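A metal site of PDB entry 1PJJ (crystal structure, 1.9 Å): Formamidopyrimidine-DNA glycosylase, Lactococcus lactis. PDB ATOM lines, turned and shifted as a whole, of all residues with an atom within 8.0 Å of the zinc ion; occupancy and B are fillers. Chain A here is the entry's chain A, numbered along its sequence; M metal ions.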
ATOM      1  N   TRP A 179       9.012   8.356 -15.853  1.00  0.00           N
ATOM      2  CA  TRP A 179      10.272   9.090 -15.989  1.00  0.00           C
ATOM      3  C   TRP A 179      10.003  10.369 -16.777  1.00  0.00           C
ATOM      4  O   TRP A 179      10.498  11.445 -16.417  1.00  0.00           O
ATOM      5  CB  TRP A 179      11.319   8.257 -16.747  1.00  0.00           C
ATOM      6  CG  TRP A 179      12.602   9.008 -17.048  1.00  0.00           C
ATOM      7  CD1 TRP A 179      13.700   9.135 -16.243  1.00  0.00           C
ATOM      8  CD2 TRP A 179      12.889   9.760 -18.241  1.00  0.00           C
ATOM      9  NE1 TRP A 179      14.661   9.906 -16.850  1.00  0.00           N
ATOM     10  CE2 TRP A 179      14.187  10.302 -18.079  1.00  0.00           C
ATOM     11  CE3 TRP A 179      12.191  10.023 -19.418  1.00  0.00           C
ATOM     12  CZ2 TRP A 179      14.800  11.093 -19.059  1.00  0.00           C
ATOM     13  CZ3 TRP A 179      12.795  10.808 -20.398  1.00  0.00           C
ATOM     14  CH2 TRP A 179      14.097  11.331 -20.210  1.00  0.00           C
ATOM     15  N   LYS A 182       8.358  12.832 -14.649  1.00  0.00           N
ATOM     16  CA  LYS A 182       9.130  13.118 -13.442  1.00  0.00           C
ATOM     17  C   LYS A 182       8.399  12.771 -12.143  1.00  0.00           C
ATOM     18  O   LYS A 182       8.357  13.559 -11.205  1.00  0.00           O
ATOM     19  CB  LYS A 182       9.542  14.592 -13.447  1.00  0.00           C
ATOM     20  CG  LYS A 182      10.364  14.986 -14.679  1.00  0.00           C
ATOM     21  CD  LYS A 182      10.622  16.479 -14.749  1.00  0.00           C
ATOM     22  CE  LYS A 182      11.342  16.841 -16.043  1.00  0.00           C
ATOM     23  NZ  LYS A 182      11.566  18.311 -16.204  1.00  0.00           N
ATOM     24  N   VAL A 237      14.607   4.639 -19.603  1.00  0.00           N
ATOM     25  CA  VAL A 237      14.936   4.004 -18.333  1.00  0.00           C
ATOM     26  C   VAL A 237      14.766   2.493 -18.239  1.00  0.00           C
ATOM     27  O   VAL A 237      15.564   1.823 -17.587  1.00  0.00           O
ATOM     28  CB  VAL A 237      14.127   4.634 -17.168  1.00  0.00           C
ATOM     29  CG1 VAL A 237      14.569   6.074 -16.947  1.00  0.00           C
ATOM     30  CG2 VAL A 237      12.630   4.580 -17.473  1.00  0.00           C
ATOM     31  N   LYS A 244      23.362   6.336 -17.630  1.00  0.00           N
ATOM     32  CA  LYS A 244      23.103   7.728 -17.255  1.00  0.00           C
ATOM     33  C   LYS A 244      21.774   8.258 -17.787  1.00  0.00           C
ATOM     34  O   LYS A 244      21.386   7.965 -18.912  1.00  0.00           O
ATOM     35  CB  LYS A 244      24.231   8.628 -17.792  1.00  0.00           C
ATOM     36  CG  LYS A 244      25.633   8.059 -17.620  1.00  0.00           C
ATOM     37  CD  LYS A 244      26.201   8.303 -16.233  1.00  0.00           C
ATOM     38  CE  LYS A 244      26.562   9.767 -16.037  1.00  0.00           C
ATOM     39  NZ  LYS A 244      27.458  10.282 -17.103  1.00  0.00           N
ATOM     40  N   CYS A 245      21.081   9.025 -16.954  1.00  0.00           N
ATOM     41  CA  CYS A 245      19.815   9.624 -17.349  1.00  0.00           C
ATOM     42  C   CYS A 245      20.133  10.651 -18.433  1.00  0.00           C
ATOM     43  O   CYS A 245      21.095  11.404 -18.312  1.00  0.00           O
ATOM     44  CB  CYS A 245      19.155  10.306 -16.157  1.00  0.00           C
ATOM     45  SG  CYS A 245      17.737  11.336 -16.560  1.00  0.00           S
ATOM     46  N   SER A 246      19.332  10.672 -19.495  1.00  0.00           N
ATOM     47  CA  SER A 246      19.563  11.599 -20.594  1.00  0.00           C
ATOM     48  C   SER A 246      19.252  13.058 -20.270  1.00  0.00           C
ATOM     49  O   SER A 246      19.607  13.961 -21.033  1.00  0.00           O
ATOM     50  CB  SER A 246      18.751  11.184 -21.819  1.00  0.00           C
ATOM     51  OG  SER A 246      17.358  11.337 -21.577  1.00  0.00           O
ATOM     52  N   ARG A 247      18.593  13.307 -19.139  1.00  0.00           N
ATOM     53  CA  ARG A 247      18.252  14.673 -18.755  1.00  0.00           C
ATOM     54  C   ARG A 247      19.220  15.291 -17.764  1.00  0.00           C
ATOM     55  O   ARG A 247      19.697  16.411 -17.970  1.00  0.00           O
ATOM     56  CB  ARG A 247      16.841  14.743 -18.165  1.00  0.00           C
ATOM     57  CG  ARG A 247      15.731  14.791 -19.193  1.00  0.00           C
ATOM     58  CD  ARG A 247      14.366  15.017 -18.540  1.00  0.00           C
ATOM     59  NE  ARG A 247      14.152  14.067 -17.448  1.00  0.00           N
ATOM     60  CZ  ARG A 247      12.985  13.511 -17.160  1.00  0.00           C
ATOM     61  NH1 ARG A 247      11.911  13.800 -17.880  1.00  0.00           N
ATOM     62  NH2 ARG A 247      12.890  12.650 -16.152  1.00  0.00           N
ATOM     63  N   CYS A 248      19.514  14.583 -16.678  1.00  0.00           N
ATOM     64  CA  CYS A 248      20.398  15.112 -15.649  1.00  0.00           C
ATOM     65  C   CYS A 248      21.761  14.461 -15.557  1.00  0.00           C
ATOM     66  O   CYS A 248      22.714  15.070 -15.081  1.00  0.00           O
ATOM     67  CB  CYS A 248      19.711  15.024 -14.288  1.00  0.00           C
ATOM     68  SG  CYS A 248      19.637  13.351 -13.643  1.00  0.00           S
ATOM     69  N   GLY A 249      21.858  13.199 -15.996  1.00  0.00           N
ATOM     70  CA  GLY A 249      23.129  12.519 -15.957  1.00  0.00           C
ATOM     71  C   GLY A 249      23.317  11.555 -14.798  1.00  0.00           C
ATOM     72  O   GLY A 249      24.350  10.890 -14.718  1.00  0.00           O
ATOM     73  N   ALA A 250      22.343  11.470 -13.895  1.00  0.00           N
ATOM     74  CA  ALA A 250      22.450  10.544 -12.768  1.00  0.00           C
ATOM     75  C   ALA A 250      22.254   9.121 -13.272  1.00  0.00           C
ATOM     76  O   ALA A 250      21.637   8.900 -14.316  1.00  0.00           O
ATOM     77  CB  ALA A 250      21.416  10.872 -11.716  1.00  0.00           C
ATOM     78  N   GLU A 251      22.776   8.137 -12.531  1.00  0.00           N
ATOM     79  CA  GLU A 251      22.624   6.741 -12.934  1.00  0.00           C
ATOM     80  C   GLU A 251      21.218   6.216 -12.704  1.00  0.00           C
ATOM     81  O   GLU A 251      20.643   6.419 -11.636  1.00  0.00           O
ATOM     82  CB  GLU A 251      23.592   5.831 -12.179  1.00  0.00           C
ATOM     83  CG  GLU A 251      25.004   5.811 -12.718  1.00  0.00           C
ATOM     84  CD  GLU A 251      25.781   4.601 -12.247  1.00  0.00           C
ATOM     85  OE1 GLU A 251      26.979   4.504 -12.560  1.00  0.00           O
ATOM     86  OE2 GLU A 251      25.192   3.738 -11.562  1.00  0.00           O
ATOM     87  N   ILE A 252      20.676   5.550 -13.710  1.00  0.00           N
ATOM     88  CA  ILE A 252      19.346   4.973 -13.585  1.00  0.00           C
ATOM     89  C   ILE A 252      19.437   3.818 -12.590  1.00  0.00           C
ATOM     90  O   ILE A 252      20.337   2.978 -12.687  1.00  0.00           O
ATOM     91  CB  ILE A 252      18.843   4.446 -14.942  1.00  0.00           C
ATOM     92  CG1 ILE A 252      18.683   5.609 -15.924  1.00  0.00           C
ATOM     93  CG2 ILE A 252      17.529   3.683 -14.761  1.00  0.00           C
ATOM     94  CD1 ILE A 252      17.777   6.731 -15.423  1.00  0.00           C
ATOM     95  N   PHE A 264      14.163   3.832 -12.689  1.00  0.00           N
ATOM     96  CA  PHE A 264      13.894   5.263 -12.551  1.00  0.00           C
ATOM     97  C   PHE A 264      15.161   6.081 -12.272  1.00  0.00           C
ATOM     98  O   PHE A 264      16.189   5.532 -11.870  1.00  0.00           O
ATOM     99  CB  PHE A 264      12.909   5.479 -11.395  1.00  0.00           C
ATOM    100  CG  PHE A 264      13.527   5.293 -10.035  1.00  0.00           C
ATOM    101  CD1 PHE A 264      13.852   6.404  -9.250  1.00  0.00           C
ATOM    102  CD2 PHE A 264      13.836   4.021  -9.551  1.00  0.00           C
ATOM    103  CE1 PHE A 264      14.473   6.244  -8.010  1.00  0.00           C
ATOM    104  CE2 PHE A 264      14.462   3.853  -8.314  1.00  0.00           C
ATOM    105  CZ  PHE A 264      14.772   4.969  -7.536  1.00  0.00           C
ATOM    106  N   CYS A 265      15.065   7.393 -12.494  1.00  0.00           N
ATOM    107  CA  CYS A 265      16.165   8.316 -12.209  1.00  0.00           C
ATOM    108  C   CYS A 265      15.855   8.938 -10.847  1.00  0.00           C
ATOM    109  O   CYS A 265      14.830   9.613 -10.689  1.00  0.00           O
ATOM    110  CB  CYS A 265      16.260   9.422 -13.262  1.00  0.00           C
ATOM    111  SG  CYS A 265      17.447  10.764 -12.830  1.00  0.00           S
ATOM    112  N   PRO A 266      16.722   8.713  -9.844  1.00  0.00           N
ATOM    113  CA  PRO A 266      16.565   9.233  -8.485  1.00  0.00           C
ATOM    114  C   PRO A 266      16.576  10.758  -8.385  1.00  0.00           C
ATOM    115  O   PRO A 266      16.127  11.323  -7.383  1.00  0.00           O
ATOM    116  CB  PRO A 266      17.734   8.604  -7.730  1.00  0.00           C
ATOM    117  CG  PRO A 266      18.075   7.392  -8.527  1.00  0.00           C
ATOM    118  CD  PRO A 266      17.934   7.892  -9.945  1.00  0.00           C
ATOM    119  N   VAL A 267      17.086  11.435  -9.411  1.00  0.00           N
ATOM    120  CA  VAL A 267      17.135  12.891  -9.413  1.00  0.00           C
ATOM    121  C   VAL A 267      15.861  13.463 -10.028  1.00  0.00           C
ATOM    122  O   VAL A 267      15.170  14.271  -9.405  1.00  0.00           O
ATOM    123  CB  VAL A 267      18.368  13.399 -10.216  1.00  0.00           C
ATOM    124  CG1 VAL A 267      18.267  14.899 -10.433  1.00  0.00           C
ATOM    125  CG2 VAL A 267      19.646  13.057  -9.456  1.00  0.00           C
ATOM    126  N   CYS A 268      15.555  13.027 -11.245  1.00  0.00           N
ATOM    127  CA  CYS A 268      14.365  13.485 -11.957  1.00  0.00           C
ATOM    128  C   CYS A 268      13.057  13.039 -11.326  1.00  0.00           C
ATOM    129  O   CYS A 268      12.028  13.713 -11.467  1.00  0.00           O
ATOM    130  CB  CYS A 268      14.416  13.004 -13.405  1.00  0.00           C
ATOM    131  SG  CYS A 268      15.690  13.800 -14.418  1.00  0.00           S
ATOM    132  N   GLN A 269      13.076  11.908 -10.625  1.00  0.00           N
ATOM    133  CA  GLN A 269      11.880  11.380  -9.997  1.00  0.00           C
ATOM    134  C   GLN A 269      12.039  11.338  -8.475  1.00  0.00           C
ATOM    135  O   GLN A 269      12.285  10.285  -7.888  1.00  0.00           O
ATOM    136  CB  GLN A 269      11.597   9.971 -10.556  1.00  0.00           C
ATOM    137  CG  GLN A 269      11.230   9.973 -12.042  1.00  0.00           C
ATOM    138  CD  GLN A 269      11.295   8.598 -12.692  1.00  0.00           C
ATOM    139  OE1 GLN A 269      12.325   8.221 -13.258  1.00  0.00           O
ATOM    140  NE2 GLN A 269      10.207   7.851 -12.596  1.00  0.00           N
HETATM  141 ZN    ZN M   1      17.526  12.310 -14.385  1.00  0.00          ZN
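SG of Cys 248 lies close to N of Ala 250. N of Cys 265 lies within hydrogen-bond range of OE1 of Gln 269 (3.0 Å). The backbone NH (N) of Cys 245 lies within hydrogen-bond range of the backbone carbonyl oxygen (O) of Ala 250 (2.7 Å). N of Arg 247 sits close to SG of Cys 245, at 3.4 Å. The side-chain sulfur (SG) of Cys 268 sits close to the guanidinium group (NE) of Arg 247. N of Val 267 lies close to SG of Cys 265. SG of Cys 245 lies close to NE1 of Trp 179 (3.4 Å).
The zinc ion is bound by SG of Cys 265, SG of Cys 268, SG of Cys 245 and SG of Cys 248.
Within 4 Å of the zinc ion: Cys 245, Cys 248, Cys 265 and Cys 268.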
